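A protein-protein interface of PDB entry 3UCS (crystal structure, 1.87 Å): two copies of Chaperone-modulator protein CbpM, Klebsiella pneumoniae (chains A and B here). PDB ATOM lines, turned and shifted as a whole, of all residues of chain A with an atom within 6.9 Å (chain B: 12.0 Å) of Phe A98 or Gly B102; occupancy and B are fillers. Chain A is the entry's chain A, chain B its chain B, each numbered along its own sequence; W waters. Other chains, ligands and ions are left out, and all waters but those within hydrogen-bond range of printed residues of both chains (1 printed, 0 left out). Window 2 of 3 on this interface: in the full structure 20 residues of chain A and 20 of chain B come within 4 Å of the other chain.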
ATOM      1  N   GLN A  93      15.932  19.448 -11.845  1.00  0.00           N
ATOM      2  CA  GLN A  93      16.503  20.744 -11.469  1.00  0.00           C
ATOM      3  C   GLN A  93      16.229  21.823 -12.505  1.00  0.00           C
ATOM      4  O   GLN A  93      15.963  22.973 -12.146  1.00  0.00           O
ATOM      5  CB  GLN A  93      18.008  20.638 -11.240  1.00  0.00           C
ATOM      6  CG  GLN A  93      18.358  19.949  -9.950  1.00  0.00           C
ATOM      7  CD  GLN A  93      19.868  19.903  -9.728  1.00  0.00           C
ATOM      8  OE1 GLN A  93      20.363  19.026  -9.037  1.00  0.00           O
ATOM      9  NE2 GLN A  93      20.599  20.836 -10.340  1.00  0.00           N
ATOM     10  N   ARG A  94      16.294  21.468 -13.789  1.00  0.00           N
ATOM     11  CA  ARG A  94      16.015  22.440 -14.844  1.00  0.00           C
ATOM     12  C   ARG A  94      14.555  22.912 -14.830  1.00  0.00           C
ATOM     13  O   ARG A  94      14.280  24.078 -15.100  1.00  0.00           O
ATOM     14  CB  ARG A  94      16.379  21.871 -16.220  1.00  0.00           C
ATOM     15  CG  ARG A  94      17.886  21.729 -16.400  1.00  0.00           C
ATOM     16  CD  ARG A  94      18.234  21.008 -17.707  1.00  0.00           C
ATOM     17  NE  ARG A  94      19.685  20.804 -17.782  1.00  0.00           N
ATOM     18  CZ  ARG A  94      20.269  19.786 -18.415  1.00  0.00           C
ATOM     19  NH1 ARG A  94      19.526  18.865 -19.044  1.00  0.00           N
ATOM     20  NH2 ARG A  94      21.594  19.681 -18.402  1.00  0.00           N
ATOM     21  N   LEU A  95      13.639  21.997 -14.529  1.00  0.00           N
ATOM     22  CA  LEU A  95      12.211  22.330 -14.387  1.00  0.00           C
ATOM     23  C   LEU A  95      12.025  23.301 -13.214  1.00  0.00           C
ATOM     24  O   LEU A  95      11.330  24.327 -13.337  1.00  0.00           O
ATOM     25  CB  LEU A  95      11.379  21.046 -14.186  1.00  0.00           C
ATOM     26  CG  LEU A  95      11.157  20.237 -15.460  1.00  0.00           C
ATOM     27  CD1 LEU A  95      10.668  18.793 -15.149  1.00  0.00           C
ATOM     28  CD2 LEU A  95      10.140  20.990 -16.313  1.00  0.00           C
ATOM     29  N   ALA A  96      12.677  23.015 -12.082  1.00  0.00           N
ATOM     30  CA  ALA A  96      12.613  23.934 -10.923  1.00  0.00           C
ATOM     31  C   ALA A  96      13.171  25.326 -11.257  1.00  0.00           C
ATOM     32  O   ALA A  96      12.590  26.367 -10.874  1.00  0.00           O
ATOM     33  CB  ALA A  96      13.346  23.335  -9.691  1.00  0.00           C
ATOM     34  N   ARG A  97      14.289  25.343 -11.978  1.00  0.00           N
ATOM     35  CA  ARG A  97      14.926  26.598 -12.387  1.00  0.00           C
ATOM     36  C   ARG A  97      13.972  27.398 -13.262  1.00  0.00           C
ATOM     37  O   ARG A  97      13.861  28.622 -13.112  1.00  0.00           O
ATOM     38  CB  ARG A  97      16.207  26.324 -13.176  1.00  0.00           C
ATOM     39  CG  ARG A  97      16.891  27.594 -13.723  1.00  0.00           C
ATOM     40  CD  ARG A  97      18.294  27.270 -14.238  1.00  0.00           C
ATOM     41  NE  ARG A  97      18.238  26.451 -15.454  1.00  0.00           N
ATOM     42  CZ  ARG A  97      19.314  25.999 -16.098  1.00  0.00           C
ATOM     43  NH1 ARG A  97      20.538  26.278 -15.629  1.00  0.00           N
ATOM     44  NH2 ARG A  97      19.165  25.279 -17.203  1.00  0.00           N
ATOM     45  N   PHE A  98      13.287  26.715 -14.174  1.00  0.00           N
ATOM     46  CA  PHE A  98      12.295  27.410 -15.022  1.00  0.00           C
ATOM     47  C   PHE A  98      11.162  28.005 -14.187  1.00  0.00           C
ATOM     48  O   PHE A  98      10.834  29.197 -14.346  1.00  0.00           O
ATOM     49  CB  PHE A  98      11.702  26.513 -16.102  1.00  0.00           C
ATOM     50  CG  PHE A  98      10.549  27.159 -16.836  1.00  0.00           C
ATOM     51  CD1 PHE A  98      10.787  27.969 -17.937  1.00  0.00           C
ATOM     52  CD2 PHE A  98       9.239  26.988 -16.388  1.00  0.00           C
ATOM     53  CE1 PHE A  98       9.729  28.582 -18.614  1.00  0.00           C
ATOM     54  CE2 PHE A  98       8.158  27.621 -17.051  1.00  0.00           C
ATOM     55  CZ  PHE A  98       8.409  28.406 -18.155  1.00  0.00           C
ATOM     56  N   LEU A  99      10.572  27.180 -13.315  1.00  0.00           N
ATOM     57  CA  LEU A  99       9.467  27.615 -12.466  1.00  0.00           C
ATOM     58  C   LEU A  99       9.819  28.787 -11.561  1.00  0.00           C
ATOM     59  O   LEU A  99       8.936  29.612 -11.220  1.00  0.00           O
ATOM     60  CB  LEU A  99       8.913  26.449 -11.637  1.00  0.00           C
ATOM     61  CG  LEU A  99       8.237  25.378 -12.504  1.00  0.00           C
ATOM     62  CD1 LEU A  99       8.055  24.097 -11.693  1.00  0.00           C
ATOM     63  CD2 LEU A  99       6.883  25.906 -13.087  1.00  0.00           C
ATOM     64  N   ALA A 100      11.092  28.864 -11.174  1.00  0.00           N
ATOM     65  CA  ALA A 100      11.557  29.924 -10.291  1.00  0.00           C
ATOM     66  C   ALA A 100      12.028  31.195 -11.015  1.00  0.00           C
ATOM     67  O   ALA A 100      12.510  32.122 -10.374  1.00  0.00           O
ATOM     68  CB  ALA A 100      12.688  29.398  -9.395  1.00  0.00           C
ATOM     69  N   HIS A 101      11.924  31.254 -12.337  1.00  0.00           N
ATOM     70  CA  HIS A 101      12.543  32.403 -13.029  1.00  0.00           C
ATOM     71  C   HIS A 101      11.591  33.573 -13.278  1.00  0.00           C
ATOM     72  O   HIS A 101      10.497  33.617 -12.700  1.00  0.00           O
ATOM     73  CB  HIS A 101      13.289  31.963 -14.286  1.00  0.00           C
ATOM     74  CG  HIS A 101      14.726  31.605 -14.029  1.00  0.00           C
ATOM     75  ND1 HIS A 101      15.218  31.349 -12.762  1.00  0.00           N
ATOM     76  CD2 HIS A 101      15.772  31.442 -14.879  1.00  0.00           C
ATOM     77  CE1 HIS A 101      16.509  31.077 -12.839  1.00  0.00           C
ATOM     78  NE2 HIS A 101      16.871  31.127 -14.112  1.00  0.00           N
ATOM     79  N   LEU B  91       9.964  14.267 -18.721  1.00  0.00           N
ATOM     80  CA  LEU B  91      10.440  15.506 -18.126  1.00  0.00           C
ATOM     81  C   LEU B  91      11.025  16.396 -19.203  1.00  0.00           C
ATOM     82  O   LEU B  91      10.852  17.598 -19.135  1.00  0.00           O
ATOM     83  CB  LEU B  91      11.489  15.253 -17.041  1.00  0.00           C
ATOM     84  CG  LEU B  91      11.050  14.478 -15.797  1.00  0.00           C
ATOM     85  CD1 LEU B  91      12.277  14.351 -14.852  1.00  0.00           C
ATOM     86  CD2 LEU B  91       9.881  15.196 -15.097  1.00  0.00           C
ATOM     87  N   GLN B  92      11.722  15.809 -20.181  1.00  0.00           N
ATOM     88  CA  GLN B  92      12.270  16.581 -21.301  1.00  0.00           C
ATOM     89  C   GLN B  92      11.143  17.247 -22.083  1.00  0.00           C
ATOM     90  O   GLN B  92      11.260  18.404 -22.470  1.00  0.00           O
ATOM     91  CB  GLN B  92      13.101  15.692 -22.241  1.00  0.00           C
ATOM     92  CG  GLN B  92      14.079  16.461 -23.139  1.00  0.00           C
ATOM     93  CD  GLN B  92      15.362  16.875 -22.404  1.00  0.00           C
ATOM     94  OE1 GLN B  92      16.274  16.058 -22.202  1.00  0.00           O
ATOM     95  NE2 GLN B  92      15.449  18.151 -22.032  1.00  0.00           N
ATOM     96  N   GLN B  93      10.063  16.509 -22.327  1.00  0.00           N
ATOM     97  CA  GLN B  93       8.908  17.069 -23.048  1.00  0.00           C
ATOM     98  C   GLN B  93       8.233  18.184 -22.240  1.00  0.00           C
ATOM     99  O   GLN B  93       7.841  19.214 -22.801  1.00  0.00           O
ATOM    100  CB  GLN B  93       7.898  15.973 -23.411  1.00  0.00           C
ATOM    101  CG  GLN B  93       8.291  15.142 -24.623  1.00  0.00           C
ATOM    102  CD  GLN B  93       7.206  14.146 -25.048  1.00  0.00           C
ATOM    103  OE1 GLN B  93       6.607  13.481 -24.215  1.00  0.00           O
ATOM    104  NE2 GLN B  93       6.965  14.040 -26.349  1.00  0.00           N
ATOM    105  N   ARG B  94       8.112  17.979 -20.928  1.00  0.00           N
ATOM    106  CA  ARG B  94       7.493  18.966 -20.041  1.00  0.00           C
ATOM    107  C   ARG B  94       8.309  20.242 -20.046  1.00  0.00           C
ATOM    108  O   ARG B  94       7.747  21.323 -20.126  1.00  0.00           O
ATOM    109  CB  ARG B  94       7.357  18.434 -18.606  1.00  0.00           C
ATOM    110  CG  ARG B  94       6.573  19.361 -17.664  1.00  0.00           C
ATOM    111  CD  ARG B  94       6.492  18.817 -16.230  1.00  0.00           C
ATOM    112  NE  ARG B  94       5.921  17.474 -16.200  1.00  0.00           N
ATOM    113  CZ  ARG B  94       6.133  16.587 -15.229  1.00  0.00           C
ATOM    114  NH1 ARG B  94       6.891  16.902 -14.179  1.00  0.00           N
ATOM    115  NH2 ARG B  94       5.581  15.385 -15.313  1.00  0.00           N
ATOM    116  N   LEU B  95       9.635  20.113 -19.966  1.00  0.00           N
ATOM    117  CA  LEU B  95      10.539  21.274 -19.985  1.00  0.00           C
ATOM    118  C   LEU B  95      10.416  22.028 -21.304  1.00  0.00           C
ATOM    119  O   LEU B  95      10.357  23.260 -21.313  1.00  0.00           O
ATOM    120  CB  LEU B  95      11.995  20.843 -19.749  1.00  0.00           C
ATOM    121  CG  LEU B  95      13.095  21.917 -19.691  1.00  0.00           C
ATOM    122  CD1 LEU B  95      12.907  22.854 -18.486  1.00  0.00           C
ATOM    123  CD2 LEU B  95      14.470  21.242 -19.607  1.00  0.00           C
ATOM    124  N   ALA B  96      10.350  21.291 -22.411  1.00  0.00           N
ATOM    125  CA  ALA B  96      10.153  21.921 -23.737  1.00  0.00           C
ATOM    126  C   ALA B  96       8.814  22.663 -23.831  1.00  0.00           C
ATOM    127  O   ALA B  96       8.737  23.745 -24.413  1.00  0.00           O
ATOM    128  CB  ALA B  96      10.261  20.862 -24.856  1.00  0.00           C
ATOM    129  N   ARG B  97       7.767  22.064 -23.261  1.00  0.00           N
ATOM    130  CA  ARG B  97       6.426  22.658 -23.217  1.00  0.00           C
ATOM    131  C   ARG B  97       6.435  23.938 -22.388  1.00  0.00           C
ATOM    132  O   ARG B  97       5.898  24.968 -22.809  1.00  0.00           O
ATOM    133  CB  ARG B  97       5.439  21.659 -22.618  1.00  0.00           C
ATOM    134  CG  ARG B  97       3.974  22.153 -22.525  1.00  0.00           C
ATOM    135  CD  ARG B  97       3.006  20.960 -22.356  1.00  0.00           C
ATOM    136  NE  ARG B  97       3.305  20.076 -21.209  1.00  0.00           N
ATOM    137  CZ  ARG B  97       3.022  20.362 -19.934  1.00  0.00           C
ATOM    138  NH1 ARG B  97       2.466  21.527 -19.617  1.00  0.00           N
ATOM    139  NH2 ARG B  97       3.299  19.490 -18.962  1.00  0.00           N
ATOM    140  N   PHE B  98       7.063  23.868 -21.216  1.00  0.00           N
ATOM    141  CA  PHE B  98       7.238  25.038 -20.335  1.00  0.00           C
ATOM    142  C   PHE B  98       7.997  26.139 -21.076  1.00  0.00           C
ATOM    143  O   PHE B  98       7.546  27.287 -21.115  1.00  0.00           O
ATOM    144  CB  PHE B  98       8.007  24.648 -19.062  1.00  0.00           C
ATOM    145  CG  PHE B  98       7.191  23.878 -18.047  1.00  0.00           C
ATOM    146  CD1 PHE B  98       7.685  23.694 -16.752  1.00  0.00           C
ATOM    147  CD2 PHE B  98       5.937  23.357 -18.359  1.00  0.00           C
ATOM    148  CE1 PHE B  98       6.946  22.986 -15.797  1.00  0.00           C
ATOM    149  CE2 PHE B  98       5.201  22.661 -17.412  1.00  0.00           C
ATOM    150  CZ  PHE B  98       5.715  22.472 -16.130  1.00  0.00           C
ATOM    151  N   LEU B  99       9.143  25.786 -21.660  1.00  0.00           N
ATOM    152  CA  LEU B  99       9.978  26.757 -22.358  1.00  0.00           C
ATOM    153  C   LEU B  99       9.255  27.400 -23.545  1.00  0.00           C
ATOM    154  O   LEU B  99       9.449  28.588 -23.820  1.00  0.00           O
ATOM    155  CB  LEU B  99      11.306  26.147 -22.807  1.00  0.00           C
ATOM    156  CG  LEU B  99      12.370  25.887 -21.732  1.00  0.00           C
ATOM    157  CD1 LEU B  99      13.546  25.123 -22.330  1.00  0.00           C
ATOM    158  CD2 LEU B  99      12.823  27.205 -21.108  1.00  0.00           C
ATOM    159  N   ALA B 100       8.404  26.630 -24.221  1.00  0.00           N
ATOM    160  CA  ALA B 100       7.572  27.170 -25.316  1.00  0.00           C
ATOM    161  C   ALA B 100       6.522  28.171 -24.804  1.00  0.00           C
ATOM    162  O   ALA B 100       6.237  29.177 -25.474  1.00  0.00           O
ATOM    163  CB  ALA B 100       6.905  26.037 -26.098  1.00  0.00           C
ATOM    164  N   HIS B 101       5.962  27.880 -23.626  1.00  0.00           N
ATOM    165  CA  HIS B 101       4.984  28.741 -22.953  1.00  0.00           C
ATOM    166  C   HIS B 101       5.687  30.019 -22.490  1.00  0.00           C
ATOM    167  O   HIS B 101       5.169  31.126 -22.675  1.00  0.00           O
ATOM    168  CB  HIS B 101       4.369  27.990 -21.760  1.00  0.00           C
ATOM    169  CG  HIS B 101       3.516  28.833 -20.853  1.00  0.00           C
ATOM    170  ND1 HIS B 101       4.037  29.808 -20.022  1.00  0.00           N
ATOM    171  CD2 HIS B 101       2.185  28.798 -20.597  1.00  0.00           C
ATOM    172  CE1 HIS B 101       3.059  30.361 -19.325  1.00  0.00           C
ATOM    173  NE2 HIS B 101       1.925  29.766 -19.653  1.00  0.00           N
ATOM    174  N   GLY B 102       6.861  29.836 -21.876  1.00  0.00           N
ATOM    175  CA  GLY B 102       7.679  30.943 -21.390  1.00  0.00           C
ATOM    176  C   GLY B 102       7.279  31.407 -20.001  1.00  0.00           C
ATOM    177  O   GLY B 102       7.929  32.298 -19.425  1.00  0.00           O
ATOM    178  OXT GLY B 102       6.302  30.903 -19.423  1.00  0.00           O
HETATM  179  O   HOH W   1      17.254  19.593 -20.774  1.00  0.00           O
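Arg A94 touches Leu B95, but with the chains exchanged Leu A95 does not touch Arg B94 (4.1 Å).
Leu B95 touches its own counterpart, Leu A95.
Phe A98 touches its own counterpart, Phe B98.
Phe A98 touches Leu B99, and with the chains exchanged Leu A99 touches Phe B98.
Among the printed residues, merely in contact across the chains: Phe A98 with Phe B98 (3.3 Å), Phe A98 with Gly B102 (3.5 Å), Leu A95 with Phe B98 (3.7 Å), Leu A95 with Leu B91 (3.7 Å), Leu A95 with Leu B95 (3.7 Å), Phe A98 with Leu B99 (3.8 Å), Arg A94 with Leu B95 (3.9 Å) and Leu A99 with Phe B98 (3.98 Å).
Of the printed residues of chain B, Arg A94 touches Leu B95.
Of the printed residues of chain B, Leu A95 touches Leu B91, Leu B95 and Phe B98.
No residue of chain B comes within 4 Å of Ala A96.
No residue of chain B comes within 4 Å of Arg A97.
Of chain B, only Phe B98 (3.3 Å), Leu B99 (3.8 Å) and Gly B102 (3.5 Å) come within 4 Å of Phe A98.
No residue of chain B comes within 4 Å of His A101.
Printed residues of chain A within 4 Å of Leu B91: Leu A95 (3.7 Å).
Gln B92 touches none of the printed residues of chain A.
Printed residues of chain A within 4 Å of Leu B95: Arg A94 (3.9 Å) and Leu A95 (3.7 Å).
Of chain A, only Phe A98 comes within 4 Å of Gly B102.
The nearest residue of chain B that does not touch Phe A98 is Leu B95 (4.5 Å).
Water W1 lies within hydrogen-bond range of NE2 of Gln B92 (2.6 Å) and NH1 of Arg A94 (2.9 Å).
Of the 9 printed residues of chain A, 4 touch a printed residue of chain B.
Hydrophobic or aromatic side chains of chain A that line the printed part of chain B: Leu A95, Phe A98 and Leu A99.
Printed residues of chain B that touch a printed residue of chain A: Leu B91, Leu B95, Phe B98, Leu B99 and Gly B102.
Hydrophobic or aromatic side chains of chain B within 4 Å of the printed part of chain A: Leu B91, Leu B95, Phe B98 and Leu B99.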
